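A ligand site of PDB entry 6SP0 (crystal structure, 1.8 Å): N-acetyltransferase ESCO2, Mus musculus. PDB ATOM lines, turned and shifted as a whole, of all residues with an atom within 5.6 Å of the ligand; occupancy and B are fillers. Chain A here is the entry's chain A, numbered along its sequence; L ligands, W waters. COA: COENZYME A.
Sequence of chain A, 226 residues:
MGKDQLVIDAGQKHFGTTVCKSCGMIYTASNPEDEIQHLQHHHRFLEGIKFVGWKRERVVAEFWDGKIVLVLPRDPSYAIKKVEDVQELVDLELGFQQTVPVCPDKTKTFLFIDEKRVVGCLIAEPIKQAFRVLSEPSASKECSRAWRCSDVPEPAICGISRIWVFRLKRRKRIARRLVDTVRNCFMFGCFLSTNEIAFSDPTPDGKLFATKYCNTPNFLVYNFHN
Merely in contact with the ligand: Glu 93, Leu 94, Gln 98, Trp 164, Arg 170, Ile 174, Pro 202, Gly 206, Leu 208, Phe 209 and Lys 212.
Within 4 Å of the ligand: Glu 93, Leu 94, Gln 98, Ile 163, Trp 164, Val 165, Arg 170, Arg 171, Lys 172, Arg 173, Ile 174, Ala 175, Arg 176, Pro 202, Thr 203, Asp 205, Gly 206, Leu 208, Phe 209 and Lys 212.
Water W8 bridges an oxygen (O8A) of the ligand (2.6 Å) and the backbone carbonyl oxygen of Arg 171 (3.1 Å).
Water W5 bridges O2B of the ligand and NZ of Lys 212.
Water W9 lies within hydrogen-bond range of the side-chain amide oxygen of Gln 98, the backbone NH of Ile 163 and a sulfur (S1P) of the ligand.
Water W3 lies within hydrogen-bond range of NH1 of Arg 171 and N6A of the ligand.
Water W12 bridges the guanidinium group of Arg 176 and an oxygen (O3B) of the ligand.
The side-chain hydroxyl (OG1) of Thr 203 sits at hydrogen-bond distance from the backbone NH (N) of Gly 206, at 3.0 Å.
The backbone carbonyl oxygen (O) of Val 165 lies within hydrogen-bond range of the guanidinium group (NE) of Arg 170, 2.8 Å away.
The guanidinium group (NE) of Arg 177 is in hydrogen-bond range of the backbone carbonyl oxygen (O) of Arg 173, at 3.0 Å.
The side-chain carboxylate (OE2) of Glu 93 lies within salt-bridge range of the guanidinium group (NH2) of Arg 170, at 2.7 Å.
NH2 of Arg 177 is in hydrogen-bond range of O of Lys 172, at 2.9 Å.
NE1 of Trp 164 sits at hydrogen-bond distance from OE1 of Glu 93 (2.8 Å).
The backbone carbonyl oxygen (O) of Asp 201 is in hydrogen-bond range of the side-chain amide nitrogen (NE2) of Gln 98, 3.2 Å away.
O4A of the ligand is in hydrogen-bond range of N of Arg 171 (2.7 Å).
The guanidinium group (NH2) of Arg 171 is in salt-bridge range of an oxygen (O9A) of the ligand.
The backbone NH (N) of Thr 203 lies close to a sulfur (S1P) of the ligand.
The side-chain hydroxyl of Thr 203 sits at hydrogen-bond distance from an oxygen (O5P) of the ligand, 2.7 Å away.
The backbone carbonyl oxygen (O) of Ile 163 is in hydrogen-bond range of a nitrogen (N4P) of the ligand (2.8 Å).
The backbone NH (N) of Arg 176 sits at hydrogen-bond distance from an oxygen (O2A) of the ligand (2.8 Å).
An oxygen (O9P) of the ligand sits at hydrogen-bond distance from the backbone NH (N) of Val 165, at 2.9 Å.
The backbone NH (N) of Arg 173 is in hydrogen-bond range of an oxygen (O1A) of the ligand (2.9 Å).
The backbone NH of Ala 175 sits at hydrogen-bond distance from an oxygen (O5A) of the ligand, at 3.0 Å.
The side-chain carboxylate of Asp 205 is in hydrogen-bond range of a nitrogen (N8P) of the ligand (3.1 Å).
The backbone NH of Lys 172 sits at hydrogen-bond distance from an oxygen (O1A) of the ligand.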
ATOM      1  N   VAL A  90       5.534 -14.623  17.320  1.00  0.00           N
ATOM      2  CA  VAL A  90       5.727 -13.254  16.876  1.00  0.00           C
ATOM      3  C   VAL A  90       5.506 -13.142  15.366  1.00  0.00           C
ATOM      4  O   VAL A  90       4.909 -12.169  14.889  1.00  0.00           O
ATOM      5  CB  VAL A  90       7.124 -12.773  17.278  1.00  0.00           C
ATOM      6  CG1 VAL A  90       7.381 -11.353  16.736  1.00  0.00           C
ATOM      7  CG2 VAL A  90       7.227 -12.805  18.804  1.00  0.00           C
ATOM      8  N   GLU A  93       1.856 -12.944  14.738  1.00  0.00           N
ATOM      9  CA  GLU A  93       1.275 -11.658  15.098  1.00  0.00           C
ATOM     10  C   GLU A  93       1.634 -10.589  14.078  1.00  0.00           C
ATOM     11  O   GLU A  93       0.782  -9.771  13.706  1.00  0.00           O
ATOM     12  CB  GLU A  93       1.765 -11.258  16.513  1.00  0.00           C
ATOM     13  CG  GLU A  93       1.228  -9.897  16.887  1.00  0.00           C
ATOM     14  CD  GLU A  93       1.667  -9.467  18.304  1.00  0.00           C
ATOM     15  OE1 GLU A  93       1.921 -10.347  19.192  1.00  0.00           O
ATOM     16  OE2 GLU A  93       1.747  -8.232  18.499  1.00  0.00           O
ATOM     17  N   LEU A  94       2.886 -10.558  13.630  1.00  0.00           N
ATOM     18  CA  LEU A  94       3.295  -9.544  12.663  1.00  0.00           C
ATOM     19  C   LEU A  94       2.628  -9.799  11.313  1.00  0.00           C
ATOM     20  O   LEU A  94       2.287  -8.861  10.594  1.00  0.00           O
ATOM     21  CB  LEU A  94       4.808  -9.539  12.481  1.00  0.00           C
ATOM     22  CG  LEU A  94       5.590  -9.051  13.719  1.00  0.00           C
ATOM     23  CD1 LEU A  94       7.091  -9.121  13.480  1.00  0.00           C
ATOM     24  CD2 LEU A  94       5.159  -7.639  14.029  1.00  0.00           C
ATOM     25  N   GLN A  98       9.830 -11.192   9.211  1.00  0.00           N
ATOM     26  CA  GLN A  98      10.794 -10.099   9.362  1.00  0.00           C
ATOM     27  C   GLN A  98      12.182 -10.618   9.011  1.00  0.00           C
ATOM     28  O   GLN A  98      12.481 -11.810   9.156  1.00  0.00           O
ATOM     29  CB  GLN A  98      10.768  -9.545  10.796  1.00  0.00           C
ATOM     30  CG  GLN A  98      11.047  -8.025  10.889  1.00  0.00           C
ATOM     31  CD  GLN A  98      10.979  -7.486  12.332  1.00  0.00           C
ATOM     32  OE1 GLN A  98      10.903  -8.246  13.299  1.00  0.00           O
ATOM     33  NE2 GLN A  98      10.988  -6.152  12.473  1.00  0.00           N
ATOM     34  N   ILE A 163      12.278  -7.396  18.292  1.00  0.00           N
ATOM     35  CA  ILE A 163      11.877  -7.011  19.663  1.00  0.00           C
ATOM     36  C   ILE A 163      10.366  -7.127  19.749  1.00  0.00           C
ATOM     37  O   ILE A 163       9.637  -6.685  18.833  1.00  0.00           O
ATOM     38  CB  ILE A 163      12.409  -5.594  20.056  1.00  0.00           C
ATOM     39  CG1 ILE A 163      12.151  -5.290  21.524  1.00  0.00           C
ATOM     40  CG2 ILE A 163      11.860  -4.466  19.099  1.00  0.00           C
ATOM     41  CD1 ILE A 163      12.855  -3.979  22.018  1.00  0.00           C
ATOM     42  N   TRP A 164       9.887  -7.814  20.792  1.00  0.00           N
ATOM     43  CA  TRP A 164       8.453  -8.037  20.928  1.00  0.00           C
ATOM     44  C   TRP A 164       8.099  -8.108  22.408  1.00  0.00           C
ATOM     45  O   TRP A 164       8.861  -8.685  23.193  1.00  0.00           O
ATOM     46  CB  TRP A 164       8.047  -9.357  20.268  1.00  0.00           C
ATOM     47  CG  TRP A 164       6.669  -9.871  20.592  1.00  0.00           C
ATOM     48  CD1 TRP A 164       5.504  -9.603  19.920  1.00  0.00           C
ATOM     49  CD2 TRP A 164       6.341 -10.823  21.596  1.00  0.00           C
ATOM     50  NE1 TRP A 164       4.462 -10.297  20.479  1.00  0.00           N
ATOM     51  CE2 TRP A 164       4.948 -11.031  21.534  1.00  0.00           C
ATOM     52  CE3 TRP A 164       7.074 -11.439  22.625  1.00  0.00           C
ATOM     53  CZ2 TRP A 164       4.280 -11.912  22.422  1.00  0.00           C
ATOM     54  CZ3 TRP A 164       6.408 -12.329  23.487  1.00  0.00           C
ATOM     55  CH2 TRP A 164       5.035 -12.552  23.386  1.00  0.00           C
ATOM     56  N   VAL A 165       6.933  -7.580  22.749  1.00  0.00           N
ATOM     57  CA  VAL A 165       6.375  -7.679  24.084  1.00  0.00           C
ATOM     58  C   VAL A 165       4.937  -8.181  23.949  1.00  0.00           C
ATOM     59  O   VAL A 165       4.175  -7.683  23.125  1.00  0.00           O
ATOM     60  CB  VAL A 165       6.441  -6.316  24.811  1.00  0.00           C
ATOM     61  CG1 VAL A 165       5.698  -6.355  26.173  1.00  0.00           C
ATOM     62  CG2 VAL A 165       7.917  -5.946  25.024  1.00  0.00           C
ATOM     63  N   PHE A 166       4.577  -9.175  24.762  1.00  0.00           N
ATOM     64  CA  PHE A 166       3.208  -9.647  24.795  1.00  0.00           C
ATOM     65  C   PHE A 166       2.209  -8.497  24.935  1.00  0.00           C
ATOM     66  O   PHE A 166       2.406  -7.587  25.747  1.00  0.00           O
ATOM     67  CB  PHE A 166       3.090 -10.620  25.976  1.00  0.00           C
ATOM     68  CG  PHE A 166       1.679 -11.130  26.214  1.00  0.00           C
ATOM     69  CD1 PHE A 166       0.970 -11.736  25.203  1.00  0.00           C
ATOM     70  CD2 PHE A 166       1.102 -11.028  27.485  1.00  0.00           C
ATOM     71  CE1 PHE A 166      -0.329 -12.226  25.426  1.00  0.00           C
ATOM     72  CE2 PHE A 166      -0.180 -11.501  27.726  1.00  0.00           C
ATOM     73  CZ  PHE A 166      -0.902 -12.106  26.675  1.00  0.00           C
ATOM     74  N   LYS A 169       1.040  -6.930  28.146  1.00  0.00           N
ATOM     75  CA  LYS A 169       2.086  -6.417  29.010  1.00  0.00           C
ATOM     76  C   LYS A 169       2.817  -5.220  28.412  1.00  0.00           C
ATOM     77  O   LYS A 169       3.915  -4.893  28.886  1.00  0.00           O
ATOM     78  CB  LYS A 169       3.090  -7.518  29.326  1.00  0.00           C
ATOM     79  CG  LYS A 169       2.514  -8.718  30.092  1.00  0.00           C
ATOM     80  CD  LYS A 169       2.279  -8.346  31.538  1.00  0.00           C
ATOM     81  CE  LYS A 169       3.559  -8.026  32.199  1.00  0.00           C
ATOM     82  NZ  LYS A 169       3.498  -8.365  33.673  1.00  0.00           N
ATOM     83  N   ARG A 170       2.257  -4.586  27.403  1.00  0.00           N
ATOM     84  CA  ARG A 170       2.935  -3.446  26.777  1.00  0.00           C
ATOM     85  C   ARG A 170       2.786  -2.170  27.589  1.00  0.00           C
ATOM     86  O   ARG A 170       1.919  -2.059  28.454  1.00  0.00           O
ATOM     87  CB  ARG A 170       2.405  -3.216  25.356  1.00  0.00           C
ATOM     88  CG  ARG A 170       2.905  -4.317  24.423  1.00  0.00           C
ATOM     89  CD  ARG A 170       2.363  -4.201  22.996  1.00  0.00           C
ATOM     90  NE  ARG A 170       2.695  -5.475  22.360  1.00  0.00           N
ATOM     91  CZ  ARG A 170       2.145  -5.961  21.257  1.00  0.00           C
ATOM     92  NH1 ARG A 170       1.256  -5.246  20.566  1.00  0.00           N
ATOM     93  NH2 ARG A 170       2.491  -7.184  20.837  1.00  0.00           N
ATOM     94  N   ARG A 171       3.685  -1.224  27.322  1.00  0.00           N
ATOM     95  CA  ARG A 171       3.728   0.077  28.002  1.00  0.00           C
ATOM     96  C   ARG A 171       3.958  -0.099  29.505  1.00  0.00           C
ATOM     97  O   ARG A 171       3.442   0.647  30.336  1.00  0.00           O
ATOM     98  CB  ARG A 171       2.473   0.893  27.726  1.00  0.00           C
ATOM     99  CG  ARG A 171       2.123   1.028  26.237  1.00  0.00           C
ATOM    100  CD  ARG A 171       3.206   1.781  25.442  1.00  0.00           C
ATOM    101  NE  ARG A 171       3.274   3.225  25.714  1.00  0.00           N
ATOM    102  CZ  ARG A 171       2.543   4.160  25.083  1.00  0.00           C
ATOM    103  NH1 ARG A 171       1.654   3.846  24.122  1.00  0.00           N
ATOM    104  NH2 ARG A 171       2.696   5.439  25.410  1.00  0.00           N
ATOM    105  N   LYS A 172       4.783  -1.085  29.822  1.00  0.00           N
ATOM    106  CA  LYS A 172       5.239  -1.398  31.162  1.00  0.00           C
ATOM    107  C   LYS A 172       6.756  -1.475  31.219  1.00  0.00           C
ATOM    108  O   LYS A 172       7.311  -2.082  32.166  1.00  0.00           O
ATOM    109  CB  LYS A 172       4.604  -2.708  31.655  1.00  0.00           C
ATOM    110  CG  LYS A 172       3.096  -2.639  31.827  1.00  0.00           C
ATOM    111  CD  LYS A 172       2.505  -4.023  32.018  1.00  0.00           C
ATOM    112  CE  LYS A 172       0.983  -4.035  31.827  1.00  0.00           C
ATOM    113  NZ  LYS A 172       0.305  -3.203  32.843  1.00  0.00           N
ATOM    114  N   ARG A 173       7.445  -0.848  30.263  1.00  0.00           N
ATOM    115  CA  ARG A 173       8.894  -0.718  30.228  1.00  0.00           C
ATOM    116  C   ARG A 173       9.600  -2.019  29.957  1.00  0.00           C
ATOM    117  O   ARG A 173      10.805  -2.111  30.195  1.00  0.00           O
ATOM    118  CB  ARG A 173       9.449  -0.116  31.554  1.00  0.00           C
ATOM    119  CG  ARG A 173       8.756   1.222  31.897  1.00  0.00           C
ATOM    120  CD  ARG A 173       9.411   1.892  33.108  1.00  0.00           C
ATOM    121  NE  ARG A 173       9.106   1.214  34.369  1.00  0.00           N
ATOM    122  CZ  ARG A 173       7.931   1.276  34.992  1.00  0.00           C
ATOM    123  NH1 ARG A 173       6.929   1.978  34.472  1.00  0.00           N
ATOM    124  NH2 ARG A 173       7.757   0.651  36.176  1.00  0.00           N
ATOM    125  N   ILE A 174       8.883  -3.059  29.517  1.00  0.00           N
ATOM    126  CA  ILE A 174       9.586  -4.321  29.232  1.00  0.00           C
ATOM    127  C   ILE A 174      10.564  -4.142  28.068  1.00  0.00           C
ATOM    128  O   ILE A 174      11.731  -4.515  28.162  1.00  0.00           O
ATOM    129  CB  ILE A 174       8.577  -5.445  28.983  1.00  0.00           C
ATOM    130  CG1 ILE A 174       7.927  -5.848  30.306  1.00  0.00           C
ATOM    131  CG2 ILE A 174       9.295  -6.678  28.470  1.00  0.00           C
ATOM    132  CD1 ILE A 174       6.707  -6.782  30.127  1.00  0.00           C
ATOM    133  N   ALA A 175      10.121  -3.557  26.956  1.00  0.00           N
ATOM    134  CA  ALA A 175      11.044  -3.342  25.845  1.00  0.00           C
ATOM    135  C   ALA A 175      12.193  -2.404  26.243  1.00  0.00           C
ATOM    136  O   ALA A 175      13.346  -2.636  25.903  1.00  0.00           O
ATOM    137  CB  ALA A 175      10.301  -2.794  24.606  1.00  0.00           C
ATOM    138  N   ARG A 176      11.896  -1.352  27.011  1.00  0.00           N
ATOM    139  CA  ARG A 176      12.995  -0.473  27.427  1.00  0.00           C
ATOM    140  C   ARG A 176      14.041  -1.237  28.228  1.00  0.00           C
ATOM    141  O   ARG A 176      15.251  -1.058  28.025  1.00  0.00           O
ATOM    142  CB  ARG A 176      12.405   0.698  28.240  1.00  0.00           C
ATOM    143  CG  ARG A 176      13.443   1.495  28.980  1.00  0.00           C
ATOM    144  CD  ARG A 176      12.734   2.576  29.832  1.00  0.00           C
ATOM    145  NE  ARG A 176      12.013   3.549  29.039  1.00  0.00           N
ATOM    146  CZ  ARG A 176      12.597   4.564  28.405  1.00  0.00           C
ATOM    147  NH1 ARG A 176      13.921   4.686  28.478  1.00  0.00           N
ATOM    148  NH2 ARG A 176      11.885   5.438  27.715  1.00  0.00           N
ATOM    149  N   ARG A 177      13.599  -2.126  29.111  1.00  0.00           N
ATOM    150  CA  ARG A 177      14.540  -2.861  29.933  1.00  0.00           C
ATOM    151  C   ARG A 177      15.286  -3.918  29.135  1.00  0.00           C
ATOM    152  O   ARG A 177      16.445  -4.209  29.440  1.00  0.00           O
ATOM    153  CB  ARG A 177      13.819  -3.515  31.114  1.00  0.00           C
ATOM    154  CG  ARG A 177      13.531  -2.477  32.180  1.00  0.00           C
ATOM    155  CD  ARG A 177      12.714  -3.112  33.281  1.00  0.00           C
ATOM    156  NE  ARG A 177      11.280  -3.164  32.982  1.00  0.00           N
ATOM    157  CZ  ARG A 177      10.447  -3.810  33.770  1.00  0.00           C
ATOM    158  NH1 ARG A 177      10.943  -4.416  34.870  1.00  0.00           N
ATOM    159  NH2 ARG A 177       9.158  -3.849  33.483  1.00  0.00           N
ATOM    160  N   PHE A 199      18.042  -0.567  14.761  1.00  0.00           N
ATOM    161  CA  PHE A 199      16.828  -1.362  14.751  1.00  0.00           C
ATOM    162  C   PHE A 199      16.583  -1.912  13.359  1.00  0.00           C
ATOM    163  O   PHE A 199      16.561  -1.148  12.392  1.00  0.00           O
ATOM    164  CB  PHE A 199      15.605  -0.536  15.201  1.00  0.00           C
ATOM    165  CG  PHE A 199      15.643  -0.136  16.670  1.00  0.00           C
ATOM    166  CD1 PHE A 199      16.389   0.966  17.082  1.00  0.00           C
ATOM    167  CD2 PHE A 199      14.965  -0.893  17.627  1.00  0.00           C
ATOM    168  CE1 PHE A 199      16.429   1.330  18.436  1.00  0.00           C
ATOM    169  CE2 PHE A 199      15.021  -0.525  18.995  1.00  0.00           C
ATOM    170  CZ  PHE A 199      15.739   0.568  19.386  1.00  0.00           C
ATOM    171  N   SER A 200      16.397  -3.214  13.271  1.00  0.00           N
ATOM    172  CA  SER A 200      16.187  -3.849  11.971  1.00  0.00           C
ATOM    173  C   SER A 200      14.767  -3.582  11.508  1.00  0.00           C
ATOM    174  O   SER A 200      13.814  -3.872  12.231  1.00  0.00           O
ATOM    175  CB  SER A 200      16.430  -5.347  12.106  1.00  0.00           C
ATOM    176  OG  SER A 200      16.001  -6.007  10.906  1.00  0.00           O
ATOM    177  N   ASP A 201      14.626  -3.019  10.295  1.00  0.00           N
ATOM    178  CA  ASP A 201      13.360  -2.989   9.572  1.00  0.00           C
ATOM    179  C   ASP A 201      12.163  -2.686  10.485  1.00  0.00           C
ATOM    180  O   ASP A 201      11.304  -3.554  10.674  1.00  0.00           O
ATOM    181  CB  ASP A 201      13.162  -4.318   8.847  1.00  0.00           C
ATOM    182  CG  ASP A 201      12.001  -4.274   7.841  1.00  0.00           C
ATOM    183  OD1 ASP A 201      11.749  -3.181   7.269  1.00  0.00           O
ATOM    184  OD2 ASP A 201      11.363  -5.327   7.636  1.00  0.00           O
ATOM    185  N   PRO A 202      12.116  -1.510  11.121  1.00  0.00           N
ATOM    186  CA  PRO A 202      11.132  -1.304  12.194  1.00  0.00           C
ATOM    187  C   PRO A 202       9.701  -1.220  11.674  1.00  0.00           C
ATOM    188  O   PRO A 202       9.420  -0.666  10.613  1.00  0.00           O
ATOM    189  CB  PRO A 202      11.561   0.009  12.850  1.00  0.00           C
ATOM    190  CG  PRO A 202      12.493   0.645  11.906  1.00  0.00           C
ATOM    191  CD  PRO A 202      13.077  -0.400  11.041  1.00  0.00           C
ATOM    192  N   THR A 203       8.796  -1.805  12.459  1.00  0.00           N
ATOM    193  CA  THR A 203       7.358  -1.649  12.349  1.00  0.00           C
ATOM    194  C   THR A 203       6.933  -0.266  12.850  1.00  0.00           C
ATOM    195  O   THR A 203       7.729   0.458  13.458  1.00  0.00           O
ATOM    196  CB  THR A 203       6.649  -2.713  13.187  1.00  0.00           C
ATOM    197  OG1 THR A 203       6.963  -2.495  14.572  1.00  0.00           O
ATOM    198  CG2 THR A 203       7.039  -4.143  12.790  1.00  0.00           C
ATOM    199  N   ASP A 205       4.973   0.358  15.463  1.00  0.00           N
ATOM    200  CA  ASP A 205       5.224   0.252  16.897  1.00  0.00           C
ATOM    201  C   ASP A 205       6.694   0.443  17.218  1.00  0.00           C
ATOM    202  O   ASP A 205       7.046   1.182  18.138  1.00  0.00           O
ATOM    203  CB  ASP A 205       4.775  -1.115  17.423  1.00  0.00           C
ATOM    204  CG  ASP A 205       3.279  -1.203  17.695  1.00  0.00           C
ATOM    205  OD1 ASP A 205       2.575  -0.205  17.405  1.00  0.00           O
ATOM    206  OD2 ASP A 205       2.820  -2.274  18.183  1.00  0.00           O
ATOM    207  N   GLY A 206       7.571  -0.253  16.468  1.00  0.00           N
ATOM    208  CA  GLY A 206       8.998  -0.146  16.747  1.00  0.00           C
ATOM    209  C   GLY A 206       9.527   1.248  16.548  1.00  0.00           C
ATOM    210  O   GLY A 206      10.420   1.702  17.265  1.00  0.00           O
ATOM    211  N   LYS A 207       8.995   1.967  15.541  1.00  0.00           N
ATOM    212  CA  LYS A 207       9.450   3.330  15.295  1.00  0.00           C
ATOM    213  C   LYS A 207       9.051   4.257  16.438  1.00  0.00           C
ATOM    214  O   LYS A 207       9.863   5.083  16.846  1.00  0.00           O
ATOM    215  CB  LYS A 207       8.883   3.862  13.961  1.00  0.00           C
ATOM    216  CG  LYS A 207       9.475   3.180  12.744  1.00  0.00           C
ATOM    217  CD  LYS A 207       8.927   3.803  11.455  1.00  0.00           C
ATOM    218  CE  LYS A 207       8.971   2.810  10.282  1.00  0.00           C
ATOM    219  NZ  LYS A 207       8.510   3.423   8.986  1.00  0.00           N
ATOM    220  N   LEU A 208       7.832   4.100  16.970  1.00  0.00           N
ATOM    221  CA  LEU A 208       7.404   4.914  18.106  1.00  0.00           C
ATOM    222  C   LEU A 208       8.241   4.594  19.338  1.00  0.00           C
ATOM    223  O   LEU A 208       8.627   5.485  20.094  1.00  0.00           O
ATOM    224  CB  LEU A 208       5.938   4.674  18.411  1.00  0.00           C
ATOM    225  CG  LEU A 208       4.917   5.298  17.435  1.00  0.00           C
ATOM    226  CD1 LEU A 208       3.544   4.693  17.559  1.00  0.00           C
ATOM    227  CD2 LEU A 208       4.870   6.793  17.726  1.00  0.00           C
ATOM    228  N   PHE A 209       8.536   3.298  19.534  1.00  0.00           N
ATOM    229  CA  PHE A 209       9.389   2.904  20.658  1.00  0.00           C
ATOM    230  C   PHE A 209      10.790   3.462  20.507  1.00  0.00           C
ATOM    231  O   PHE A 209      11.350   4.033  21.469  1.00  0.00           O
ATOM    232  CB  PHE A 209       9.436   1.376  20.761  1.00  0.00           C
ATOM    233  CG  PHE A 209      10.486   0.894  21.703  1.00  0.00           C
ATOM    234  CD1 PHE A 209      10.280   1.060  23.088  1.00  0.00           C
ATOM    235  CD2 PHE A 209      11.679   0.375  21.242  1.00  0.00           C
ATOM    236  CE1 PHE A 209      11.253   0.623  24.003  1.00  0.00           C
ATOM    237  CE2 PHE A 209      12.701  -0.022  22.160  1.00  0.00           C
ATOM    238  CZ  PHE A 209      12.475   0.108  23.549  1.00  0.00           C
ATOM    239  N   LYS A 212      11.364   7.236  21.113  1.00  0.00           N
ATOM    240  CA  LYS A 212      11.417   7.591  22.516  1.00  0.00           C
ATOM    241  C   LYS A 212      12.671   7.025  23.178  1.00  0.00           C
ATOM    242  O   LYS A 212      13.350   7.742  23.924  1.00  0.00           O
ATOM    243  CB  LYS A 212      10.175   7.071  23.219  1.00  0.00           C
ATOM    244  CG  LYS A 212      10.185   7.409  24.715  1.00  0.00           C
ATOM    245  CD  LYS A 212      10.539   8.897  24.921  1.00  0.00           C
ATOM    246  CE  LYS A 212       9.547   9.585  25.855  1.00  0.00           C
ATOM    247  NZ  LYS A 212       9.416   8.914  27.193  1.00  0.00           N
ATOM    248  N   TYR A 213      13.002   5.762  22.899  1.00  0.00           N
ATOM    249  CA  TYR A 213      14.128   5.143  23.602  1.00  0.00           C
ATOM    250  C   TYR A 213      15.428   5.870  23.311  1.00  0.00           C
ATOM    251  O   TYR A 213      16.253   6.097  24.207  1.00  0.00           O
ATOM    252  CB  TYR A 213      14.256   3.651  23.240  1.00  0.00           C
ATOM    253  CG  TYR A 213      15.345   2.999  24.086  1.00  0.00           C
ATOM    254  CD1 TYR A 213      15.042   2.420  25.321  1.00  0.00           C
ATOM    255  CD2 TYR A 213      16.656   3.005  23.681  1.00  0.00           C
ATOM    256  CE1 TYR A 213      16.024   1.855  26.108  1.00  0.00           C
ATOM    257  CE2 TYR A 213      17.668   2.454  24.465  1.00  0.00           C
ATOM    258  CZ  TYR A 213      17.327   1.888  25.677  1.00  0.00           C
ATOM    259  OH  TYR A 213      18.327   1.350  26.471  1.00  0.00           O
HETATM  260  N1A COA L   1       2.732   3.723  20.662  1.00  0.00           N
HETATM  261  C2A COA L   1       3.447   4.924  21.090  1.00  0.00           C
HETATM  262  N3A COA L   1       4.527   4.898  21.829  1.00  0.00           N
HETATM  263  C4A COA L   1       4.991   3.872  22.196  1.00  0.00           C
HETATM  264  C5A COA L   1       4.435   2.551  21.873  1.00  0.00           C
HETATM  265  C6A COA L   1       3.310   2.442  21.096  1.00  0.00           C
HETATM  266  N6A COA L   1       2.686   1.163  20.716  1.00  0.00           N
HETATM  267  N7A COA L   1       5.362   1.664  22.552  1.00  0.00           N
HETATM  268  C8A COA L   1       6.241   2.249  23.117  1.00  0.00           C
HETATM  269  N9A COA L   1       6.101   3.474  22.956  1.00  0.00           N
HETATM  270  C1B COA L   1       6.963   4.456  23.486  1.00  0.00           C
HETATM  271  C2B COA L   1       6.376   5.142  24.641  1.00  0.00           C
HETATM  272  O2B COA L   1       6.978   6.475  24.633  1.00  0.00           O
HETATM  273  C3B COA L   1       6.889   4.402  25.797  1.00  0.00           C
HETATM  274  O3B COA L   1       6.952   5.233  26.966  1.00  0.00           O
HETATM  275  P3B COA L   1       5.604   5.439  27.888  1.00  0.00           P
HETATM  276  O7A COA L   1       6.089   5.941  29.222  1.00  0.00           O
HETATM  277  O8A COA L   1       4.835   4.166  28.067  1.00  0.00           O
HETATM  278  O9A COA L   1       4.690   6.412  27.172  1.00  0.00           O
HETATM  279  C4B COA L   1       8.299   4.096  25.454  1.00  0.00           C
HETATM  280  O4B COA L   1       8.241   3.787  24.005  1.00  0.00           O
HETATM  281  C5B COA L   1       8.833   2.870  26.174  1.00  0.00           C
HETATM  282  O5B COA L   1       7.918   1.822  25.814  1.00  0.00           O
HETATM  283  P1A COA L   1       8.026   0.321  26.513  1.00  0.00           P
HETATM  284  O1A COA L   1       6.964   0.191  27.548  1.00  0.00           O
HETATM  285  O2A COA L   1       9.423   0.059  26.920  1.00  0.00           O
HETATM  286  O3A COA L   1       7.612  -0.595  25.178  1.00  0.00           O
HETATM  287  P2A COA L   1       6.761  -1.975  25.216  1.00  0.00           P
HETATM  288  O4A COA L   1       5.329  -1.715  25.243  1.00  0.00           O
HETATM  289  O5A COA L   1       7.260  -2.808  26.337  1.00  0.00           O
HETATM  290  O6A COA L   1       7.241  -2.605  23.794  1.00  0.00           O
HETATM  291  CBP COA L   1       7.185  -2.762  21.444  1.00  0.00           C
HETATM  292  CCP COA L   1       7.361  -1.751  22.632  1.00  0.00           C
HETATM  293  CDP COA L   1       8.202  -3.915  21.576  1.00  0.00           C
HETATM  294  CEP COA L   1       7.459  -2.006  20.123  1.00  0.00           C
HETATM  295  CAP COA L   1       5.745  -3.300  21.457  1.00  0.00           C
HETATM  296  OAP COA L   1       4.848  -2.325  21.027  1.00  0.00           O
HETATM  297  C9P COA L   1       5.547  -4.574  20.554  1.00  0.00           C
HETATM  298  O9P COA L   1       5.917  -5.684  20.817  1.00  0.00           O
HETATM  299  N8P COA L   1       4.780  -4.370  19.315  1.00  0.00           N
HETATM  300  C7P COA L   1       4.486  -5.548  18.455  1.00  0.00           C
HETATM  301  C6P COA L   1       5.708  -6.223  17.825  1.00  0.00           C
HETATM  302  C5P COA L   1       6.490  -5.152  17.087  1.00  0.00           C
HETATM  303  O5P COA L   1       6.004  -4.446  16.215  1.00  0.00           O
HETATM  304  N4P COA L   1       7.873  -5.038  17.489  1.00  0.00           N
HETATM  305  C3P COA L   1       8.768  -4.008  16.900  1.00  0.00           C
HETATM  306  C2P COA L   1       9.464  -4.574  15.695  1.00  0.00           C
HETATM  307  S1P COA L   1      10.576  -3.163  15.332  1.00  0.00           S
HETATM  308  O   HOH W   1       6.487   2.395  29.072  1.00  0.00           O
HETATM  309  O   HOH W   2       1.318  -0.770  22.829  1.00  0.00           O
HETATM  310  O   HOH W   3       0.514   1.759  23.069  1.00  0.00           O
HETATM  311  O   HOH W   4       5.404   7.711  21.718  1.00  0.00           O
HETATM  312  O   HOH W   5       6.172   8.990  26.064  1.00  0.00           O
HETATM  313  O   HOH W   6       2.812   8.043  28.289  1.00  0.00           O
HETATM  314  O   HOH W   7       3.964  -0.773  23.098  1.00  0.00           O
HETATM  315  O   HOH W   8       2.972   3.625  29.863  1.00  0.00           O
HETATM  316  O   HOH W   9      11.739  -6.543  15.511  1.00  0.00           O
HETATM  317  O   HOH W  10       6.116  -3.231  28.573  1.00  0.00           O
HETATM  318  O   HOH W  11       5.953   5.345  31.629  1.00  0.00           O
HETATM  319  O   HOH W  12       8.829   3.876  29.439  1.00  0.00           O
HETATM  320  O   HOH W  13       3.712  -4.572  14.895  1.00  0.00           O
